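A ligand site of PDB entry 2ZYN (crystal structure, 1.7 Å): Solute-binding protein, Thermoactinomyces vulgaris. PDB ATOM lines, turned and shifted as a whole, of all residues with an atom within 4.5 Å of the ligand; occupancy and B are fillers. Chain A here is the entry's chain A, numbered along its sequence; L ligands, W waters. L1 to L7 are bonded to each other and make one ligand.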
ATOM      1  N   ASN A  26      10.044  13.679   6.635  1.00  0.00           N
ATOM      2  CA  ASN A  26      10.341  13.745   8.060  1.00  0.00           C
ATOM      3  C   ASN A  26       9.064  13.766   8.912  1.00  0.00           C
ATOM      4  O   ASN A  26       8.157  14.565   8.668  1.00  0.00           O
ATOM      5  CB  ASN A  26      11.197  14.990   8.350  1.00  0.00           C
ATOM      6  CG  ASN A  26      11.662  15.062   9.800  1.00  0.00           C
ATOM      7  OD1 ASN A  26      11.766  14.045  10.491  1.00  0.00           O
ATOM      8  ND2 ASN A  26      11.956  16.275  10.258  1.00  0.00           N
ATOM      9  N   ALA A  27       9.027  12.875   9.903  1.00  0.00           N
ATOM     10  CA  ALA A  27       7.879  12.755  10.798  1.00  0.00           C
ATOM     11  C   ALA A  27       7.915  13.815  11.893  1.00  0.00           C
ATOM     12  O   ALA A  27       8.083  13.505  13.082  1.00  0.00           O
ATOM     13  CB  ALA A  27       7.833  11.345  11.402  1.00  0.00           C
ATOM     14  N   ASP A  28       7.753  15.071  11.475  1.00  0.00           N
ATOM     15  CA  ASP A  28       7.707  16.198  12.402  1.00  0.00           C
ATOM     16  C   ASP A  28       6.294  16.490  12.910  1.00  0.00           C
ATOM     17  O   ASP A  28       6.082  17.456  13.641  1.00  0.00           O
ATOM     18  CB  ASP A  28       8.377  17.458  11.802  1.00  0.00           C
ATOM     19  CG  ASP A  28       7.535  18.135  10.718  1.00  0.00           C
ATOM     20  OD1 ASP A  28       6.674  17.481  10.079  1.00  0.00           O
ATOM     21  OD2 ASP A  28       7.743  19.343  10.502  1.00  0.00           O
ATOM     22  N   GLN A  32       6.761  20.385   8.016  1.00  0.00           N
ATOM     23  CA  GLN A  32       7.507  19.707   6.949  1.00  0.00           C
ATOM     24  C   GLN A  32       6.661  18.620   6.302  1.00  0.00           C
ATOM     25  O   GLN A  32       6.623  18.504   5.072  1.00  0.00           O
ATOM     26  CB  GLN A  32       8.804  19.116   7.488  1.00  0.00           C
ATOM     27  CG  GLN A  32       9.833  20.155   7.912  1.00  0.00           C
ATOM     28  CD  GLN A  32      11.103  19.531   8.444  1.00  0.00           C
ATOM     29  OE1 GLN A  32      11.420  18.374   8.143  1.00  0.00           O
ATOM     30  NE2 GLN A  32      11.860  20.291   9.223  1.00  0.00           N
ATOM     31  N   ALA A  57      10.764   9.438  10.493  1.00  0.00           N
ATOM     32  CA  ALA A  57      11.807  10.280  11.080  1.00  0.00           C
ATOM     33  C   ALA A  57      13.022  10.449  10.179  1.00  0.00           C
ATOM     34  O   ALA A  57      13.542   9.471   9.634  1.00  0.00           O
ATOM     35  CB  ALA A  57      12.214   9.748  12.441  1.00  0.00           C
ATOM     36  N   LEU A  58      13.470  11.689  10.032  1.00  0.00           N
ATOM     37  CA  LEU A  58      14.610  12.027   9.171  1.00  0.00           C
ATOM     38  C   LEU A  58      15.798  11.077   9.337  1.00  0.00           C
ATOM     39  O   LEU A  58      16.395  10.635   8.356  1.00  0.00           O
ATOM     40  CB  LEU A  58      15.052  13.467   9.453  1.00  0.00           C
ATOM     41  CG  LEU A  58      16.126  14.104   8.565  1.00  0.00           C
ATOM     42  CD1 LEU A  58      15.552  14.486   7.192  1.00  0.00           C
ATOM     43  CD2 LEU A  58      16.719  15.319   9.251  1.00  0.00           C
ATOM     44  N   LEU A  59      16.201  10.858  10.592  1.00  0.00           N
ATOM     45  CA  LEU A  59      17.343  10.007  10.926  1.00  0.00           C
ATOM     46  C   LEU A  59      17.064   8.485  10.953  1.00  0.00           C
ATOM     47  O   LEU A  59      17.987   7.697  11.211  1.00  0.00           O
ATOM     48  CB  LEU A  59      18.011  10.523  12.223  1.00  0.00           C
ATOM     49  CG  LEU A  59      18.539  11.982  12.205  1.00  0.00           C
ATOM     50  CD1 LEU A  59      19.062  12.413  13.573  1.00  0.00           C
ATOM     51  CD2 LEU A  59      19.644  12.163  11.157  1.00  0.00           C
ATOM     52  N   LYS A  60      15.812   8.092  10.693  1.00  0.00           N
ATOM     53  CA  LYS A  60      15.456   6.682  10.620  1.00  0.00           C
ATOM     54  C   LYS A  60      15.253   6.214   9.183  1.00  0.00           C
ATOM     55  O   LYS A  60      15.223   5.002   8.917  1.00  0.00           O
ATOM     56  CB  LYS A  60      14.212   6.394  11.462  1.00  0.00           C
ATOM     57  CG  LYS A  60      14.427   6.523  12.974  1.00  0.00           C
ATOM     58  CD  LYS A  60      13.194   6.099  13.771  1.00  0.00           C
ATOM     59  CE  LYS A  60      13.067   4.579  13.861  1.00  0.00           C
ATOM     60  NZ  LYS A  60      11.860   4.151  14.621  1.00  0.00           N
ATOM     61  N   PRO A  81      19.841  14.267   5.631  1.00  0.00           N
ATOM     62  CA  PRO A  81      20.998  15.141   5.413  1.00  0.00           C
ATOM     63  C   PRO A  81      22.126  14.448   4.644  1.00  0.00           C
ATOM     64  O   PRO A  81      22.327  13.244   4.779  1.00  0.00           O
ATOM     65  CB  PRO A  81      21.449  15.499   6.833  1.00  0.00           C
ATOM     66  CG  PRO A  81      20.249  15.265   7.688  1.00  0.00           C
ATOM     67  CD  PRO A  81      19.527  14.120   7.063  1.00  0.00           C
ATOM     68  N   ASP A  83      25.278  14.069   4.708  1.00  0.00           N
ATOM     69  CA  ASP A  83      26.491  13.456   5.273  1.00  0.00           C
ATOM     70  C   ASP A  83      26.583  11.956   5.001  1.00  0.00           C
ATOM     71  O   ASP A  83      27.664  11.412   4.813  1.00  0.00           O
ATOM     72  CB  ASP A  83      26.643  13.730   6.772  1.00  0.00           C
ATOM     73  CG  ASP A  83      25.418  13.328   7.563  1.00  0.00           C
ATOM     74  OD1 ASP A  83      24.369  13.991   7.404  1.00  0.00           O
ATOM     75  OD2 ASP A  83      25.505  12.388   8.382  1.00  0.00           O
ATOM     76  N   ARG A  84      25.434  11.289   4.969  1.00  0.00           N
ATOM     77  CA  ARG A  84      25.397   9.848   4.767  1.00  0.00           C
ATOM     78  C   ARG A  84      25.108   9.431   3.323  1.00  0.00           C
ATOM     79  O   ARG A  84      24.701   8.306   3.072  1.00  0.00           O
ATOM     80  CB  ARG A  84      24.403   9.193   5.735  1.00  0.00           C
ATOM     81  CG  ARG A  84      24.816   9.258   7.197  1.00  0.00           C
ATOM     82  CD  ARG A  84      23.783   8.616   8.090  1.00  0.00           C
ATOM     83  NE  ARG A  84      23.652   7.179   7.833  1.00  0.00           N
ATOM     84  CZ  ARG A  84      22.687   6.403   8.314  1.00  0.00           C
ATOM     85  NH1 ARG A  84      21.731   6.904   9.086  1.00  0.00           N
ATOM     86  NH2 ARG A  84      22.672   5.106   8.009  1.00  0.00           N
ATOM     87  N   GLU A 129      21.358  24.354   5.656  1.00  0.00           N
ATOM     88  CA  GLU A 129      21.220  24.693   7.079  1.00  0.00           C
ATOM     89  C   GLU A 129      22.519  24.684   7.879  1.00  0.00           C
ATOM     90  O   GLU A 129      23.443  23.919   7.601  1.00  0.00           O
ATOM     91  CB  GLU A 129      20.214  23.743   7.737  1.00  0.00           C
ATOM     92  CG  GLU A 129      20.692  22.308   7.875  1.00  0.00           C
ATOM     93  CD  GLU A 129      19.573  21.304   8.124  1.00  0.00           C
ATOM     94  OE1 GLU A 129      19.895  20.118   8.319  1.00  0.00           O
ATOM     95  OE2 GLU A 129      18.392  21.702   8.138  1.00  0.00           O
ATOM     96  N   GLU A 170      22.369  20.936  22.745  1.00  0.00           N
ATOM     97  CA  GLU A 170      22.737  19.524  22.727  1.00  0.00           C
ATOM     98  C   GLU A 170      24.249  19.334  22.745  1.00  0.00           C
ATOM     99  O   GLU A 170      24.844  18.988  21.714  1.00  0.00           O
ATOM    100  CB  GLU A 170      22.134  18.847  21.503  1.00  0.00           C
ATOM    101  CG  GLU A 170      20.948  17.953  21.784  1.00  0.00           C
ATOM    102  CD  GLU A 170      20.375  17.364  20.513  1.00  0.00           C
ATOM    103  OE1 GLU A 170      19.608  18.071  19.831  1.00  0.00           O
ATOM    104  OE2 GLU A 170      20.692  16.197  20.211  1.00  0.00           O
ATOM    105  N   ASN A 173      26.098  16.068  21.622  1.00  0.00           N
ATOM    106  CA  ASN A 173      25.916  15.761  20.206  1.00  0.00           C
ATOM    107  C   ASN A 173      26.981  16.445  19.343  1.00  0.00           C
ATOM    108  O   ASN A 173      27.048  17.671  19.301  1.00  0.00           O
ATOM    109  CB  ASN A 173      24.508  16.188  19.764  1.00  0.00           C
ATOM    110  CG  ASN A 173      24.119  15.662  18.384  1.00  0.00           C
ATOM    111  OD1 ASN A 173      24.959  15.482  17.500  1.00  0.00           O
ATOM    112  ND2 ASN A 173      22.819  15.439  18.188  1.00  0.00           N
ATOM    113  N   TYR A 175      27.256  16.858  16.196  1.00  0.00           N
ATOM    114  CA  TYR A 175      26.702  17.773  15.193  1.00  0.00           C
ATOM    115  C   TYR A 175      26.668  19.204  15.720  1.00  0.00           C
ATOM    116  O   TYR A 175      26.945  20.148  14.984  1.00  0.00           O
ATOM    117  CB  TYR A 175      25.289  17.360  14.744  1.00  0.00           C
ATOM    118  CG  TYR A 175      24.707  18.331  13.754  1.00  0.00           C
ATOM    119  CD1 TYR A 175      25.094  18.315  12.415  1.00  0.00           C
ATOM    120  CD2 TYR A 175      23.783  19.296  14.157  1.00  0.00           C
ATOM    121  CE1 TYR A 175      24.589  19.217  11.499  1.00  0.00           C
ATOM    122  CE2 TYR A 175      23.257  20.216  13.239  1.00  0.00           C
ATOM    123  CZ  TYR A 175      23.665  20.160  11.920  1.00  0.00           C
ATOM    124  OH  TYR A 175      23.158  21.061  11.013  1.00  0.00           O
ATOM    125  N   TYR A 176      26.327  19.362  17.000  1.00  0.00           N
ATOM    126  CA  TYR A 176      26.218  20.663  17.633  1.00  0.00           C
ATOM    127  C   TYR A 176      27.549  21.191  18.144  1.00  0.00           C
ATOM    128  O   TYR A 176      27.804  22.400  18.087  1.00  0.00           O
ATOM    129  CB  TYR A 176      25.207  20.614  18.781  1.00  0.00           C
ATOM    130  CG  TYR A 176      23.771  20.544  18.318  1.00  0.00           C
ATOM    131  CD1 TYR A 176      23.186  19.316  17.978  1.00  0.00           C
ATOM    132  CD2 TYR A 176      23.002  21.700  18.206  1.00  0.00           C
ATOM    133  CE1 TYR A 176      21.867  19.256  17.543  1.00  0.00           C
ATOM    134  CE2 TYR A 176      21.691  21.651  17.774  1.00  0.00           C
ATOM    135  CZ  TYR A 176      21.123  20.434  17.448  1.00  0.00           C
ATOM    136  OH  TYR A 176      19.811  20.384  17.025  1.00  0.00           O
ATOM    137  N   ALA A 230      17.091  16.807  22.001  1.00  0.00           N
ATOM    138  CA  ALA A 230      16.417  17.933  21.370  1.00  0.00           C
ATOM    139  C   ALA A 230      15.180  18.402  22.138  1.00  0.00           C
ATOM    140  O   ALA A 230      14.968  19.603  22.327  1.00  0.00           O
ATOM    141  CB  ALA A 230      16.059  17.599  19.926  1.00  0.00           C
ATOM    142  N   ASP A 231      14.370  17.444  22.590  1.00  0.00           N
ATOM    143  CA  ASP A 231      13.110  17.746  23.284  1.00  0.00           C
ATOM    144  C   ASP A 231      13.295  18.519  24.581  1.00  0.00           C
ATOM    145  O   ASP A 231      12.453  19.347  24.939  1.00  0.00           O
ATOM    146  CB  ASP A 231      12.312  16.464  23.547  1.00  0.00           C
ATOM    147  CG  ASP A 231      11.661  15.904  22.299  1.00  0.00           C
ATOM    148  OD1 ASP A 231      11.168  14.760  22.348  1.00  0.00           O
ATOM    149  OD2 ASP A 231      11.633  16.611  21.257  1.00  0.00           O
ATOM    150  N   ASN A 234      14.497  22.139  23.243  1.00  0.00           N
ATOM    151  CA  ASN A 234      13.341  22.820  22.663  1.00  0.00           C
ATOM    152  C   ASN A 234      12.252  23.129  23.688  1.00  0.00           C
ATOM    153  O   ASN A 234      11.745  24.249  23.733  1.00  0.00           O
ATOM    154  CB  ASN A 234      12.751  21.995  21.515  1.00  0.00           C
ATOM    155  CG  ASN A 234      13.682  21.896  20.328  1.00  0.00           C
ATOM    156  OD1 ASN A 234      14.476  22.803  20.071  1.00  0.00           O
ATOM    157  ND2 ASN A 234      13.593  20.795  19.597  1.00  0.00           N
ATOM    158  N   ASN A 247      20.825  26.126  17.838  1.00  0.00           N
ATOM    159  CA  ASN A 247      19.947  25.284  17.042  1.00  0.00           C
ATOM    160  C   ASN A 247      19.787  25.848  15.639  1.00  0.00           C
ATOM    161  O   ASN A 247      20.295  26.938  15.341  1.00  0.00           O
ATOM    162  CB  ASN A 247      18.584  25.098  17.736  1.00  0.00           C
ATOM    163  CG  ASN A 247      18.029  23.684  17.572  1.00  0.00           C
ATOM    164  OD1 ASN A 247      18.612  22.860  16.860  1.00  0.00           O
ATOM    165  ND2 ASN A 247      16.923  23.397  18.251  1.00  0.00           N
ATOM    166  N   TRP A 250      15.229  24.815  11.421  1.00  0.00           N
ATOM    167  CA  TRP A 250      14.150  23.855  11.579  1.00  0.00           C
ATOM    168  C   TRP A 250      13.365  24.050  12.880  1.00  0.00           C
ATOM    169  O   TRP A 250      12.277  23.505  13.023  1.00  0.00           O
ATOM    170  CB  TRP A 250      14.717  22.427  11.538  1.00  0.00           C
ATOM    171  CG  TRP A 250      15.775  22.194  12.582  1.00  0.00           C
ATOM    172  CD1 TRP A 250      15.581  21.940  13.908  1.00  0.00           C
ATOM    173  CD2 TRP A 250      17.191  22.207  12.375  1.00  0.00           C
ATOM    174  NE1 TRP A 250      16.786  21.794  14.546  1.00  0.00           N
ATOM    175  CE2 TRP A 250      17.800  21.962  13.626  1.00  0.00           C
ATOM    176  CE3 TRP A 250      18.019  22.413  11.259  1.00  0.00           C
ATOM    177  CZ2 TRP A 250      19.185  21.894  13.791  1.00  0.00           C
ATOM    178  CZ3 TRP A 250      19.401  22.365  11.426  1.00  0.00           C
ATOM    179  CH2 TRP A 250      19.961  22.104  12.678  1.00  0.00           C
ATOM    180  N   LYS A 282      19.684  19.051   2.885  1.00  0.00           N
ATOM    181  CA  LYS A 282      18.635  18.035   2.827  1.00  0.00           C
ATOM    182  C   LYS A 282      18.024  18.021   1.433  1.00  0.00           C
ATOM    183  O   LYS A 282      17.551  19.046   0.943  1.00  0.00           O
ATOM    184  CB  LYS A 282      17.574  18.281   3.910  1.00  0.00           C
ATOM    185  CG  LYS A 282      18.090  18.010   5.317  1.00  0.00           C
ATOM    186  CD  LYS A 282      17.019  18.073   6.388  1.00  0.00           C
ATOM    187  CE  LYS A 282      16.674  19.504   6.757  1.00  0.00           C
ATOM    188  NZ  LYS A 282      16.264  19.630   8.176  1.00  0.00           N
ATOM    189  N   MET A 350      29.245  19.138   5.867  1.00  0.00           N
ATOM    190  CA  MET A 350      29.566  17.843   6.456  1.00  0.00           C
ATOM    191  C   MET A 350      30.219  16.961   5.402  1.00  0.00           C
ATOM    192  O   MET A 350      29.791  16.964   4.251  1.00  0.00           O
ATOM    193  CB  MET A 350      28.319  17.150   6.996  1.00  0.00           C
ATOM    194  CG  MET A 350      27.702  17.828   8.215  1.00  0.00           C
ATOM    195  SD  MET A 350      26.340  16.903   8.915  1.00  0.00           S
ATOM    196  CE  MET A 350      25.038  17.242   7.735  1.00  0.00           C
ATOM    197  N   TRP A 360      29.375   8.902  13.513  1.00  0.00           N
ATOM    198  CA  TRP A 360      28.386   9.496  14.433  1.00  0.00           C
ATOM    199  C   TRP A 360      28.140   8.761  15.746  1.00  0.00           C
ATOM    200  O   TRP A 360      28.163   9.387  16.809  1.00  0.00           O
ATOM    201  CB  TRP A 360      27.059   9.756  13.719  1.00  0.00           C
ATOM    202  CG  TRP A 360      27.159  10.785  12.632  1.00  0.00           C
ATOM    203  CD1 TRP A 360      27.037  10.570  11.287  1.00  0.00           C
ATOM    204  CD2 TRP A 360      27.389  12.192  12.787  1.00  0.00           C
ATOM    205  NE1 TRP A 360      27.178  11.755  10.610  1.00  0.00           N
ATOM    206  CE2 TRP A 360      27.394  12.765  11.501  1.00  0.00           C
ATOM    207  CE3 TRP A 360      27.597  13.027  13.901  1.00  0.00           C
ATOM    208  CZ2 TRP A 360      27.596  14.135  11.282  1.00  0.00           C
ATOM    209  CZ3 TRP A 360      27.790  14.396  13.681  1.00  0.00           C
ATOM    210  CH2 TRP A 360      27.790  14.929  12.379  1.00  0.00           C
ATOM    211  N   GLU A 361      27.904   7.455  15.683  1.00  0.00           N
ATOM    212  CA  GLU A 361      27.604   6.693  16.904  1.00  0.00           C
ATOM    213  C   GLU A 361      28.763   6.718  17.921  1.00  0.00           C
ATOM    214  O   GLU A 361      28.554   7.097  19.064  1.00  0.00           O
ATOM    215  CB  GLU A 361      27.136   5.264  16.588  1.00  0.00           C
ATOM    216  CG  GLU A 361      26.634   4.489  17.809  1.00  0.00           C
ATOM    217  CD  GLU A 361      26.093   3.114  17.468  1.00  0.00           C
ATOM    218  OE1 GLU A 361      25.240   3.014  16.558  1.00  0.00           O
ATOM    219  OE2 GLU A 361      26.507   2.127  18.117  1.00  0.00           O
ATOM    220  N   ASN A 364      29.363  10.388  19.258  1.00  0.00           N
ATOM    221  CA  ASN A 364      28.301  10.801  20.177  1.00  0.00           C
ATOM    222  C   ASN A 364      28.364  10.022  21.490  1.00  0.00           C
ATOM    223  O   ASN A 364      28.118  10.586  22.557  1.00  0.00           O
ATOM    224  CB  ASN A 364      26.910  10.673  19.530  1.00  0.00           C
ATOM    225  CG  ASN A 364      26.552  11.882  18.651  1.00  0.00           C
ATOM    226  OD1 ASN A 364      25.439  11.994  18.154  1.00  0.00           O
ATOM    227  ND2 ASN A 364      27.508  12.779  18.468  1.00  0.00           N
HETATM  228  C1  LIG L   1      15.991   9.887  18.048  1.00  0.00           C
HETATM  229  C2  LIG L   1      14.599   9.628  17.498  1.00  0.00           C
HETATM  230  C3  LIG L   1      14.204  10.682  16.494  1.00  0.00           C
HETATM  231  C4  LIG L   1      14.313  12.114  17.082  1.00  0.00           C
HETATM  232  C5  LIG L   1      15.726  12.375  17.635  1.00  0.00           C
HETATM  233  C6  LIG L   1      15.781  13.644  18.472  1.00  0.00           C
HETATM  234  O1  LIG L   1      14.521   8.355  16.872  1.00  0.00           O
HETATM  235  O2  LIG L   1      12.893  10.458  15.990  1.00  0.00           O
HETATM  236  O3  LIG L   1      14.007  13.028  16.064  1.00  0.00           O
HETATM  237  O4  LIG L   1      16.255  11.272  18.461  1.00  0.00           O
HETATM  238  O5  LIG L   1      16.856  14.396  17.954  1.00  0.00           O
HETATM  239  C1  LG2 L   2      12.739  13.691  16.260  1.00  0.00           C
HETATM  240  C2  LG2 L   2      12.008  13.907  14.957  1.00  0.00           C
HETATM  241  C3  LG2 L   2      12.773  14.867  14.020  1.00  0.00           C
HETATM  242  C4  LG2 L   2      13.153  16.221  14.680  1.00  0.00           C
HETATM  243  C5  LG2 L   2      13.690  16.004  16.179  1.00  0.00           C
HETATM  244  C6  LG2 L   2      13.557  17.247  17.066  1.00  0.00           C
HETATM  245  O1  LG2 L   2      11.724  12.679  14.254  1.00  0.00           O
HETATM  246  O2  LG2 L   2      11.989  15.104  12.844  1.00  0.00           O
HETATM  247  O3  LG2 L   2      14.204  16.746  13.878  1.00  0.00           O
HETATM  248  O4  LG2 L   2      13.048  14.915  16.935  1.00  0.00           O
HETATM  249  O5  LG2 L   2      12.202  17.677  17.059  1.00  0.00           O
HETATM  250  C1  LG3 L   3      20.436   7.502  16.167  1.00  0.00           C
HETATM  251  C2  LG3 L   3      19.087   6.823  15.931  1.00  0.00           C
HETATM  252  C3  LG3 L   3      17.963   7.882  15.868  1.00  0.00           C
HETATM  253  C4  LG3 L   3      17.938   8.734  17.153  1.00  0.00           C
HETATM  254  C5  LG3 L   3      19.357   9.352  17.372  1.00  0.00           C
HETATM  255  C6  LG3 L   3      19.440  10.204  18.683  1.00  0.00           C
HETATM  256  O1  LG3 L   3      19.158   6.036  14.762  1.00  0.00           O
HETATM  257  O2  LG3 L   3      16.679   7.319  15.655  1.00  0.00           O
HETATM  258  O3  LG3 L   3      16.924   9.696  16.973  1.00  0.00           O
HETATM  259  O4  LG3 L   3      20.429   8.347  17.342  1.00  0.00           O
HETATM  260  O5  LG3 L   3      19.457   9.333  19.836  1.00  0.00           O
HETATM  261  C1  LG4 L   4      14.274  18.224  13.846  1.00  0.00           C
HETATM  262  C2  LG4 L   4      14.587  18.684  12.419  1.00  0.00           C
HETATM  263  C3  LG4 L   4      15.914  18.091  11.996  1.00  0.00           C
HETATM  264  C4  LG4 L   4      17.074  18.473  12.974  1.00  0.00           C
HETATM  265  C5  LG4 L   4      16.685  18.101  14.440  1.00  0.00           C
HETATM  266  C6  LG4 L   4      17.606  18.721  15.492  1.00  0.00           C
HETATM  267  O1  LG4 L   4      13.554  18.340  11.515  1.00  0.00           O
HETATM  268  O2  LG4 L   4      16.260  18.485  10.658  1.00  0.00           O
HETATM  269  O3  LG4 L   4      18.255  17.801  12.561  1.00  0.00           O
HETATM  270  O4  LG4 L   4      15.340  18.585  14.726  1.00  0.00           O
HETATM  271  O5  LG4 L   4      17.173  18.362  16.780  1.00  0.00           O
HETATM  272  C1  LG5 L   5      23.482   9.818  12.366  1.00  0.00           C
HETATM  273  C2  LG5 L   5      22.491   8.840  11.792  1.00  0.00           C
HETATM  274  C3  LG5 L   5      21.334   8.599  12.764  1.00  0.00           C
HETATM  275  C4  LG5 L   5      21.807   8.188  14.210  1.00  0.00           C
HETATM  276  C5  LG5 L   5      22.925   9.161  14.690  1.00  0.00           C
HETATM  277  C6  LG5 L   5      23.695   8.721  15.953  1.00  0.00           C
HETATM  278  O1  LG5 L   5      21.991   9.251  10.515  1.00  0.00           O
HETATM  279  O2  LG5 L   5      20.378   7.694  12.305  1.00  0.00           O
HETATM  280  O3  LG5 L   5      20.651   8.389  15.020  1.00  0.00           O
HETATM  281  O4  LG5 L   5      23.940   9.389  13.665  1.00  0.00           O
HETATM  282  O5  LG5 L   5      24.242   7.412  15.709  1.00  0.00           O
HETATM  283  C1  LG6 L   6      19.437  18.574  12.570  1.00  0.00           C
HETATM  284  C2  LG6 L   6      20.045  18.410  11.155  1.00  0.00           C
HETATM  285  C3  LG6 L   6      20.821  17.052  10.969  1.00  0.00           C
HETATM  286  C4  LG6 L   6      21.645  16.621  12.201  1.00  0.00           C
HETATM  287  C5  LG6 L   6      20.800  16.709  13.500  1.00  0.00           C
HETATM  288  C6  LG6 L   6      21.606  16.336  14.746  1.00  0.00           C
HETATM  289  O1  LG6 L   6      19.025  18.524  10.133  1.00  0.00           O
HETATM  290  O2  LG6 L   6      21.753  17.164   9.899  1.00  0.00           O
HETATM  291  O3  LG6 L   6      22.110  15.285  12.043  1.00  0.00           O
HETATM  292  O4  LG6 L   6      20.254  18.024  13.674  1.00  0.00           O
HETATM  293  O5  LG6 L   6      20.705  15.988  15.774  1.00  0.00           O
HETATM  294  C1  LG7 L   7      23.519  15.112  11.864  1.00  0.00           C
HETATM  295  C2  LG7 L   7      23.730  14.203  10.661  1.00  0.00           C
HETATM  296  C3  LG7 L   7      23.127  12.823  10.911  1.00  0.00           C
HETATM  297  C4  LG7 L   7      23.628  12.193  12.255  1.00  0.00           C
HETATM  298  C5  LG7 L   7      23.485  13.195  13.418  1.00  0.00           C
HETATM  299  C6  LG7 L   7      24.183  12.746  14.689  1.00  0.00           C
HETATM  300  O1  LG7 L   7      23.210  14.776   9.470  1.00  0.00           O
HETATM  301  O2  LG7 L   7      23.283  11.924   9.854  1.00  0.00           O
HETATM  302  O3  LG7 L   7      22.810  11.090  12.526  1.00  0.00           O
HETATM  303  O4  LG7 L   7      24.033  14.487  13.058  1.00  0.00           O
HETATM  304  O5  LG7 L   7      23.691  13.491  15.782  1.00  0.00           O
HETATM  305  O   HOH W   1      25.063   6.261  13.377  1.00  0.00           O
HETATM  306  O   HOH W   2      21.562  12.127  16.857  1.00  0.00           O
HETATM  307  O   HOH W   3      11.218  19.200  12.868  1.00  0.00           O
HETATM  308  O   HOH W   4      21.992  11.633   7.077  1.00  0.00           O
HETATM  309  O   HOH W   5      25.375   7.078  10.893  1.00  0.00           O
HETATM  310  O   HOH W   6      18.886  16.314  17.925  1.00  0.00           O
HETATM  311  O   HOH W   7      16.192   4.231  14.911  1.00  0.00           O
HETATM  312  O   HOH W   8      22.528  19.559   8.885  1.00  0.00           O
HETATM  313  O   HOH W   9      11.780  18.885  19.598  1.00  0.00           O
HETATM  314  O   HOH W  10      21.441   5.233  18.515  1.00  0.00           O
HETATM  315  O   HOH W  11      16.092  20.751  17.335  1.00  0.00           O
HETATM  316  O   HOH W  12      14.996  12.002  13.171  1.00  0.00           O
HETATM  317  O   HOH W  13      18.061  14.425  20.728  1.00  0.00           O
HETATM  318  O   HOH W  14      14.559  14.553  21.561  1.00  0.00           O
HETATM  319  O   HOH W  15      20.885   5.009  12.028  1.00  0.00           O
HETATM  320  O   HOH W  16      17.977   4.299  12.211  1.00  0.00           O
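Ala 27 touches the ligand.
CB of Ala 57 touches O1 of LG2 L2 (3.5 Å).
CD2 of Leu 58 touches O2 of LG4 L4 (3.5 Å).
CG of Lys 60 touches O2 of LG3 L3, at 3.6 Å.
CB of Pro 81 touches O1 of LG7 L7, at 3.3 Å.
OE1 of Glu 170 touches O5 of LG4 L4, 3.9 Å away.
Tyr 175 touches the ligand.
CB of Ala 230 touches O5 of LG4 L4 (3.4 Å).
NE1 of Trp 250 touches C6 of LG4 L4, 3.3 Å away.
CE of Met 350 touches O1 of LG7 L7, 3.5 Å away.
CB of Trp 360 touches O4 of LG5 L5, 3.1 Å away.
CA of Glu 361 touches O5 of LG5 L5 (3.6 Å).
Within 4 Å of the ligand: Asn 26, Ala 27, Gln 32, Ala 57, Leu 58, Leu 59, Lys 60, Pro 81, Asp 83, Arg 84, Glu 129, Glu 170, Asn 173, Tyr 175, Tyr 176, Ala 230, Trp 250, Lys 282, Met 350, Trp 360, Glu 361 and Asn 364.
The nearest printed residue that does not touch the ligand is Asn 234 (4.3 Å).
OD2 of Asp 83 sits at hydrogen-bond distance from NE1 of Trp 360 (2.9 Å).
The side-chain carboxylate of Glu 129 lies within salt-bridge range of the side-chain amino group of Lys 282 (3.0 Å).
OE1 of Gln 32 sits at hydrogen-bond distance from ND2 of Asn 26 (3.0 Å).
The side-chain amide oxygen (OD1) of Asn 26 sits at hydrogen-bond distance from the backbone NH (N) of Leu 58, at 2.9 Å.
The backbone NH (N) of Tyr 175 is in hydrogen-bond range of the side-chain amide oxygen (OD1) of Asn 173 (3.0 Å).
OH of Tyr 176 lies within hydrogen-bond range of OD1 of Asn 247 (2.8 Å).
The side-chain amide nitrogen (ND2) of Asn 234 is in hydrogen-bond range of the backbone carbonyl oxygen (O) of Ala 230 (3.3 Å).
OD2 of Asp 28 is in hydrogen-bond range of N of Gln 32, at 2.9 Å.
OD1 of Asp 83 is in hydrogen-bond range of O1 of LG7 L7, 2.5 Å away.
An oxygen (O1) of LG6 L6 sits at hydrogen-bond distance from the side-chain carboxylate of Glu 129 (2.6 Å).
An oxygen (O2) of LG2 L2 sits at hydrogen-bond distance from the side-chain amide oxygen of Asn 26 (2.6 Å).
O of Leu 59 lies within hydrogen-bond range of O2 of LG5 L5 (2.6 Å).
O2 of LG4 L4 is in hydrogen-bond range of NZ of Lys 282, at 2.7 Å.
O1 of LG5 L5 sits at hydrogen-bond distance from NH1 of Arg 84 (2.8 Å).
OD1 of Asn 173 sits at hydrogen-bond distance from O5 of LG7 L7, 2.9 Å away.
The side-chain hydroxyl (OH) of Tyr 176 lies close to an oxygen (O5) of LG4 L4 (3.3 Å).
The side-chain amide oxygen (OD1) of Asn 364 lies within hydrogen-bond range of an oxygen (O5) of LG7 L7, at 3.3 Å.
An oxygen (O1) of LG4 L4 is in hydrogen-bond range of the side-chain amide nitrogen of Gln 32 (3.5 Å).
Water W8 lies within hydrogen-bond range of OH of Tyr 175 (2.7 Å), O2 of LG6 L6 (2.7 Å) and OE1 of Glu 129 (2.8 Å).
Water W6 lies within hydrogen-bond range of the side-chain carboxylate of Glu 170 and an oxygen (O5) of LIG L1.
Water W9 lies within hydrogen-bond range of the side-chain amide nitrogen of Asn 234 (2.6 Å), the side-chain carboxylate of Asp 231 (2.8 Å) and an oxygen (O5) of LG2 L2 (2.8 Å).
Water W13 lies within hydrogen-bond range of N of Ala 230, O5 of LIG L1 and OE2 of Glu 170.
Water W4 lies within hydrogen-bond range of O of Pro 81 (2.8 Å), O2 of LG7 L7 (3.1 Å) and OD1 of Asp 83 (3.4 Å).
Water W12 lies within hydrogen-bond range of the backbone NH (N) of Leu 59 (3.1 Å) and an oxygen (O3) of LIG L1 (3.2 Å).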
